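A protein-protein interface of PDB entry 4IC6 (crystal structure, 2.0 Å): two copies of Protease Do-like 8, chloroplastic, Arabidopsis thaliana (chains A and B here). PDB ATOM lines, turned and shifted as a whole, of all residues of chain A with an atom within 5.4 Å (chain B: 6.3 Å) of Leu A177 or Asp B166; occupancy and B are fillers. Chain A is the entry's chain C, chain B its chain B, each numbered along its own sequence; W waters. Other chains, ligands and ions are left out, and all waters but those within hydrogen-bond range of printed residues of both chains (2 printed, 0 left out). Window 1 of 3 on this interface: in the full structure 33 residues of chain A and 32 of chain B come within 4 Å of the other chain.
No position is printed for both chains.
The backbone carbonyl oxygen of Gly B160 sits at hydrogen-bond distance from the backbone NH of Thr B168 (2.9 Å). The backbone carbonyl oxygen of Gln A194 is in hydrogen-bond range of the backbone NH of Ser A175, 2.7 Å away. O of Arg A179 is in hydrogen-bond range of N of Gly A192 (2.8 Å). N of Phe B165 lies close to NE2 of Gln B111, 3.3 Å away. The side-chain amide oxygen (OD1) of Asn B161 sits close to the backbone carbonyl oxygen (O) of Asp B166 (3.0 Å). NE2 of Gln B111 lies close to N of Asp B166.
Among the printed residues, pairs that only touch across the chains: Ser A175 with Thr B168, Arg A179 with Thr B168, Arg A179 with Pro B162, Leu A177 with Asp B166, Arg A179 with Phe B165 and Arg A179 with Phe B163.
Of the 10 printed residues of chain B, 5 touch a printed residue of chain A. Printed residues of chain B that touch a printed residue of chain A: Pro B162, Phe B163, Phe B165, Asp B166 and Thr B168. Hydrophobic or aromatic side chains of chain B within 4 Å of the printed part of chain A: Pro B162, Phe B163 and Phe B165. Of the 12 printed residues of chain A, 3 touch a printed residue of chain B. Printed residues of chain A that touch a printed residue of chain B: Ser A175, Leu A177 and Arg A179.
The side-chain carboxylate of Asp B166 is in salt-bridge range of the guanidinium group of Arg A179 (3.0 Å).
Leu A177 touches just one residue of chain B: Asp B166. Asp B166 touches just these residues of chain A: Leu A177 (3.9 Å) and Arg A179 (2.3 Å). Printed residues of chain B within 4 Å of Arg A179: Pro B162 (3.7 Å), Phe B163 (3.96 Å), Phe B165 (3.9 Å), Asp B166 (2.3 Å) and Thr B168 (3.5 Å). Of the printed residues of chain B, Ser A175 touches Thr B168. Printed residues of chain A within 4 Å of Pro B162: Arg A179 (3.7 Å). Printed residues of chain A within 4 Å of Phe B165: Arg A179 (3.9 Å). Printed residues of chain A within 4 Å of Phe B163: Arg A179 (3.96 Å). Ile A174 touches none of the printed residues of chain B.
Water W1 lies within hydrogen-bond range of the side-chain carboxylate of Asp B166 and the backbone carbonyl oxygen of Leu A177. Water W2 lies within hydrogen-bond range of O of His B167, N of Leu A177 and OD2 of Asp B166.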
ATOM      1  N   LEU A 150      -2.296   4.718 -11.349  1.00  0.00           N
ATOM      2  CA  LEU A 150      -2.876   6.032 -11.641  1.00  0.00           C
ATOM      3  C   LEU A 150      -4.301   5.891 -12.156  1.00  0.00           C
ATOM      4  O   LEU A 150      -4.637   4.908 -12.821  1.00  0.00           O
ATOM      5  CB  LEU A 150      -2.050   6.767 -12.698  1.00  0.00           C
ATOM      6  CG  LEU A 150      -0.772   7.447 -12.234  1.00  0.00           C
ATOM      7  CD1 LEU A 150      -0.068   8.048 -13.451  1.00  0.00           C
ATOM      8  CD2 LEU A 150      -1.086   8.538 -11.220  1.00  0.00           C
ATOM      9  N   LYS A 151      -5.138   6.880 -11.858  1.00  0.00           N
ATOM     10  CA  LYS A 151      -6.496   6.894 -12.394  1.00  0.00           C
ATOM     11  C   LYS A 151      -6.730   8.169 -13.167  1.00  0.00           C
ATOM     12  O   LYS A 151      -6.286   9.237 -12.741  1.00  0.00           O
ATOM     13  CB  LYS A 151      -7.507   6.759 -11.265  1.00  0.00           C
ATOM     14  CG  LYS A 151      -7.467   5.366 -10.599  1.00  0.00           C
ATOM     15  CD  LYS A 151      -7.901   5.419  -9.157  1.00  0.00           C
ATOM     16  CE  LYS A 151      -7.964   4.003  -8.526  1.00  0.00           C
ATOM     17  NZ  LYS A 151      -9.066   3.210  -9.141  1.00  0.00           N
ATOM     18  N   VAL A 152      -7.376   8.042 -14.320  1.00  0.00           N
ATOM     19  CA  VAL A 152      -7.752   9.208 -15.089  1.00  0.00           C
ATOM     20  C   VAL A 152      -8.635  10.057 -14.191  1.00  0.00           C
ATOM     21  O   VAL A 152      -9.555   9.555 -13.532  1.00  0.00           O
ATOM     22  CB  VAL A 152      -8.496   8.803 -16.376  1.00  0.00           C
ATOM     23  CG1 VAL A 152      -8.951  10.050 -17.164  1.00  0.00           C
ATOM     24  CG2 VAL A 152      -7.584   7.936 -17.236  1.00  0.00           C
ATOM     25  N   ILE A 174      -4.836  13.894 -14.786  1.00  0.00           N
ATOM     26  CA  ILE A 174      -4.453  12.810 -15.671  1.00  0.00           C
ATOM     27  C   ILE A 174      -5.567  12.669 -16.693  1.00  0.00           C
ATOM     28  O   ILE A 174      -6.738  12.489 -16.334  1.00  0.00           O
ATOM     29  CB  ILE A 174      -4.294  11.494 -14.903  1.00  0.00           C
ATOM     30  CG1 ILE A 174      -3.225  11.667 -13.840  1.00  0.00           C
ATOM     31  CG2 ILE A 174      -3.899  10.388 -15.867  1.00  0.00           C
ATOM     32  CD1 ILE A 174      -1.876  12.022 -14.441  1.00  0.00           C
ATOM     33  N   SER A 175      -5.203  12.753 -17.964  1.00  0.00           N
ATOM     34  CA  SER A 175      -6.195  12.826 -19.029  1.00  0.00           C
ATOM     35  C   SER A 175      -6.335  11.510 -19.790  1.00  0.00           C
ATOM     36  O   SER A 175      -7.366  11.242 -20.406  1.00  0.00           O
ATOM     37  CB  SER A 175      -5.822  13.959 -19.996  1.00  0.00           C
ATOM     38  OG  SER A 175      -6.599  13.853 -21.182  1.00  0.00           O
ATOM     39  N   GLY A 176      -5.281  10.703 -19.752  1.00  0.00           N
ATOM     40  CA  GLY A 176      -5.255   9.428 -20.448  1.00  0.00           C
ATOM     41  C   GLY A 176      -4.040   8.632 -20.019  1.00  0.00           C
ATOM     42  O   GLY A 176      -3.060   9.192 -19.522  1.00  0.00           O
ATOM     43  N   LEU A 177      -4.096   7.325 -20.219  1.00  0.00           N
ATOM     44  CA  LEU A 177      -3.019   6.449 -19.753  1.00  0.00           C
ATOM     45  C   LEU A 177      -2.564   5.583 -20.919  1.00  0.00           C
ATOM     46  O   LEU A 177      -3.331   5.344 -21.849  1.00  0.00           O
ATOM     47  CB  LEU A 177      -3.533   5.571 -18.609  1.00  0.00           C
ATOM     48  CG  LEU A 177      -3.225   5.880 -17.137  1.00  0.00           C
ATOM     49  CD1 LEU A 177      -2.711   7.282 -16.912  1.00  0.00           C
ATOM     50  CD2 LEU A 177      -4.429   5.577 -16.224  1.00  0.00           C
ATOM     51  N   ASN A 178      -1.320   5.118 -20.866  1.00  0.00           N
ATOM     52  CA  ASN A 178      -0.772   4.253 -21.906  1.00  0.00           C
ATOM     53  C   ASN A 178      -0.955   4.832 -23.294  1.00  0.00           C
ATOM     54  O   ASN A 178      -1.470   4.168 -24.186  1.00  0.00           O
ATOM     55  CB  ASN A 178      -1.380   2.843 -21.829  1.00  0.00           C
ATOM     56  CG  ASN A 178      -1.117   2.163 -20.481  1.00  0.00           C
ATOM     57  OD1 ASN A 178       0.029   1.841 -20.142  1.00  0.00           O
ATOM     58  ND2 ASN A 178      -2.181   1.936 -19.712  1.00  0.00           N
ATOM     59  N   ARG A 179      -0.530   6.081 -23.469  1.00  0.00           N
ATOM     60  CA  ARG A 179      -0.609   6.756 -24.758  1.00  0.00           C
ATOM     61  C   ARG A 179       0.787   6.946 -25.334  1.00  0.00           C
ATOM     62  O   ARG A 179       1.760   7.117 -24.592  1.00  0.00           O
ATOM     63  CB  ARG A 179      -1.299   8.125 -24.594  1.00  0.00           C
ATOM     64  CG  ARG A 179      -2.832   8.111 -24.725  1.00  0.00           C
ATOM     65  CD  ARG A 179      -3.278   8.640 -26.126  1.00  0.00           C
ATOM     66  NE  ARG A 179      -4.735   8.608 -26.326  1.00  0.00           N
ATOM     67  CZ  ARG A 179      -5.532   7.673 -25.811  1.00  0.00           C
ATOM     68  NH1 ARG A 179      -5.009   6.688 -25.087  1.00  0.00           N
ATOM     69  NH2 ARG A 179      -6.845   7.712 -26.029  1.00  0.00           N
ATOM     70  N   GLY A 192       2.944   6.075 -22.311  1.00  0.00           N
ATOM     71  CA  GLY A 192       3.018   7.386 -21.706  1.00  0.00           C
ATOM     72  C   GLY A 192       1.754   7.841 -20.990  1.00  0.00           C
ATOM     73  O   GLY A 192       0.651   7.360 -21.263  1.00  0.00           O
ATOM     74  N   ILE A 193       1.934   8.774 -20.059  1.00  0.00           N
ATOM     75  CA  ILE A 193       0.834   9.389 -19.343  1.00  0.00           C
ATOM     76  C   ILE A 193       0.451  10.630 -20.135  1.00  0.00           C
ATOM     77  O   ILE A 193       1.324  11.384 -20.565  1.00  0.00           O
ATOM     78  CB  ILE A 193       1.279   9.840 -17.942  1.00  0.00           C
ATOM     79  CG1 ILE A 193       1.598   8.626 -17.069  1.00  0.00           C
ATOM     80  CG2 ILE A 193       0.189  10.698 -17.261  1.00  0.00           C
ATOM     81  CD1 ILE A 193       2.283   8.995 -15.763  1.00  0.00           C
ATOM     82  N   GLN A 194      -0.846  10.810 -20.358  1.00  0.00           N
ATOM     83  CA  GLN A 194      -1.367  12.027 -20.969  1.00  0.00           C
ATOM     84  C   GLN A 194      -1.991  12.883 -19.858  1.00  0.00           C
ATOM     85  O   GLN A 194      -2.685  12.367 -18.992  1.00  0.00           O
ATOM     86  CB  GLN A 194      -2.444  11.707 -22.018  1.00  0.00           C
ATOM     87  CG  GLN A 194      -2.959  12.970 -22.731  1.00  0.00           C
ATOM     88  CD  GLN A 194      -3.979  12.679 -23.821  1.00  0.00           C
ATOM     89  OE1 GLN A 194      -3.618  12.281 -24.930  1.00  0.00           O
ATOM     90  NE2 GLN A 194      -5.258  12.880 -23.513  1.00  0.00           N
ATOM     91  N   GLN B 111     -14.231  -3.467 -24.666  1.00  0.00           N
ATOM     92  CA  GLN B 111     -15.138  -2.820 -25.601  1.00  0.00           C
ATOM     93  C   GLN B 111     -15.594  -3.788 -26.691  1.00  0.00           C
ATOM     94  O   GLN B 111     -14.775  -4.468 -27.314  1.00  0.00           O
ATOM     95  CB  GLN B 111     -14.508  -1.565 -26.217  1.00  0.00           C
ATOM     96  CG  GLN B 111     -14.137  -0.487 -25.189  1.00  0.00           C
ATOM     97  CD  GLN B 111     -13.986   0.889 -25.802  1.00  0.00           C
ATOM     98  OE1 GLN B 111     -14.693   1.242 -26.754  1.00  0.00           O
ATOM     99  NE2 GLN B 111     -13.058   1.678 -25.263  1.00  0.00           N
ATOM    100  N   GLY B 160     -13.857  11.345 -23.777  1.00  0.00           N
ATOM    101  CA  GLY B 160     -13.776  10.772 -25.109  1.00  0.00           C
ATOM    102  C   GLY B 160     -13.517   9.276 -25.072  1.00  0.00           C
ATOM    103  O   GLY B 160     -13.122   8.714 -24.048  1.00  0.00           O
ATOM    104  N   ASN B 161     -13.755   8.640 -26.211  1.00  0.00           N
ATOM    105  CA  ASN B 161     -13.387   7.253 -26.451  1.00  0.00           C
ATOM    106  C   ASN B 161     -12.976   7.237 -27.908  1.00  0.00           C
ATOM    107  O   ASN B 161     -13.703   6.746 -28.761  1.00  0.00           O
ATOM    108  CB  ASN B 161     -14.579   6.327 -26.182  1.00  0.00           C
ATOM    109  CG  ASN B 161     -14.295   4.876 -26.516  1.00  0.00           C
ATOM    110  OD1 ASN B 161     -13.187   4.520 -26.937  1.00  0.00           O
ATOM    111  ND2 ASN B 161     -15.299   4.020 -26.313  1.00  0.00           N
ATOM    112  N   PRO B 162     -11.815   7.838 -28.204  1.00  0.00           N
ATOM    113  CA  PRO B 162     -11.472   8.113 -29.601  1.00  0.00           C
ATOM    114  C   PRO B 162     -11.061   6.875 -30.398  1.00  0.00           C
ATOM    115  O   PRO B 162     -11.229   6.864 -31.621  1.00  0.00           O
ATOM    116  CB  PRO B 162     -10.303   9.101 -29.481  1.00  0.00           C
ATOM    117  CG  PRO B 162      -9.654   8.748 -28.186  1.00  0.00           C
ATOM    118  CD  PRO B 162     -10.780   8.317 -27.268  1.00  0.00           C
ATOM    119  N   PHE B 163     -10.538   5.850 -29.731  1.00  0.00           N
ATOM    120  CA  PHE B 163     -10.043   4.677 -30.454  1.00  0.00           C
ATOM    121  C   PHE B 163     -10.674   3.341 -30.057  1.00  0.00           C
ATOM    122  O   PHE B 163     -10.338   2.309 -30.631  1.00  0.00           O
ATOM    123  CB  PHE B 163      -8.523   4.595 -30.353  1.00  0.00           C
ATOM    124  CG  PHE B 163      -7.838   5.868 -30.728  1.00  0.00           C
ATOM    125  CD1 PHE B 163      -7.988   6.397 -32.002  1.00  0.00           C
ATOM    126  CD2 PHE B 163      -7.054   6.549 -29.810  1.00  0.00           C
ATOM    127  CE1 PHE B 163      -7.364   7.580 -32.358  1.00  0.00           C
ATOM    128  CE2 PHE B 163      -6.421   7.738 -30.158  1.00  0.00           C
ATOM    129  CZ  PHE B 163      -6.580   8.255 -31.431  1.00  0.00           C
ATOM    130  N   GLY B 164     -11.577   3.351 -29.083  1.00  0.00           N
ATOM    131  CA  GLY B 164     -12.261   2.131 -28.696  1.00  0.00           C
ATOM    132  C   GLY B 164     -11.411   1.145 -27.913  1.00  0.00           C
ATOM    133  O   GLY B 164     -11.687  -0.056 -27.920  1.00  0.00           O
ATOM    134  N   PHE B 165     -10.374   1.634 -27.236  1.00  0.00           N
ATOM    135  CA  PHE B 165      -9.613   0.766 -26.334  1.00  0.00           C
ATOM    136  C   PHE B 165      -9.395   1.426 -24.986  1.00  0.00           C
ATOM    137  O   PHE B 165      -8.898   0.801 -24.065  1.00  0.00           O
ATOM    138  CB  PHE B 165      -8.274   0.328 -26.938  1.00  0.00           C
ATOM    139  CG  PHE B 165      -7.337   1.463 -27.217  1.00  0.00           C
ATOM    140  CD1 PHE B 165      -6.576   2.022 -26.198  1.00  0.00           C
ATOM    141  CD2 PHE B 165      -7.213   1.976 -28.498  1.00  0.00           C
ATOM    142  CE1 PHE B 165      -5.714   3.080 -26.452  1.00  0.00           C
ATOM    143  CE2 PHE B 165      -6.349   3.031 -28.760  1.00  0.00           C
ATOM    144  CZ  PHE B 165      -5.598   3.583 -27.735  1.00  0.00           C
ATOM    145  N   ASP B 166      -9.777   2.692 -24.871  1.00  0.00           N
ATOM    146  CA  ASP B 166      -9.696   3.382 -23.588  1.00  0.00           C
ATOM    147  C   ASP B 166     -10.593   4.607 -23.604  1.00  0.00           C
ATOM    148  O   ASP B 166     -11.352   4.812 -24.563  1.00  0.00           O
ATOM    149  CB  ASP B 166      -8.252   3.792 -23.261  1.00  0.00           C
ATOM    150  CG  ASP B 166      -7.734   4.892 -24.167  1.00  0.00           C
ATOM    151  OD1 ASP B 166      -8.528   5.455 -24.959  1.00  0.00           O
ATOM    152  OD2 ASP B 166      -6.524   5.199 -24.090  1.00  0.00           O
ATOM    153  N   HIS B 167     -10.518   5.407 -22.540  1.00  0.00           N
ATOM    154  CA  HIS B 167     -11.243   6.671 -22.499  1.00  0.00           C
ATOM    155  C   HIS B 167     -10.330   7.839 -22.116  1.00  0.00           C
ATOM    156  O   HIS B 167      -9.260   7.641 -21.548  1.00  0.00           O
ATOM    157  CB  HIS B 167     -12.420   6.581 -21.539  1.00  0.00           C
ATOM    158  CG  HIS B 167     -13.600   5.864 -22.116  1.00  0.00           C
ATOM    159  ND1 HIS B 167     -13.714   4.487 -22.106  1.00  0.00           N
ATOM    160  CD2 HIS B 167     -14.699   6.330 -22.751  1.00  0.00           C
ATOM    161  CE1 HIS B 167     -14.850   4.140 -22.689  1.00  0.00           C
ATOM    162  NE2 HIS B 167     -15.464   5.239 -23.094  1.00  0.00           N
ATOM    163  N   THR B 168     -10.761   9.050 -22.447  1.00  0.00           N
ATOM    164  CA  THR B 168      -9.980  10.250 -22.174  1.00  0.00           C
ATOM    165  C   THR B 168     -10.791  11.220 -21.372  1.00  0.00           C
ATOM    166  O   THR B 168     -12.018  11.182 -21.384  1.00  0.00           O
ATOM    167  CB  THR B 168      -9.567  10.990 -23.460  1.00  0.00           C
ATOM    168  OG1 THR B 168     -10.740  11.345 -24.207  1.00  0.00           O
ATOM    169  CG2 THR B 168      -8.638  10.121 -24.313  1.00  0.00           C
HETATM  170  O   HOH W   1      -4.976   3.317 -23.135  1.00  0.00           O
HETATM  171  O   HOH W   2      -6.916   6.440 -21.134  1.00  0.00           O
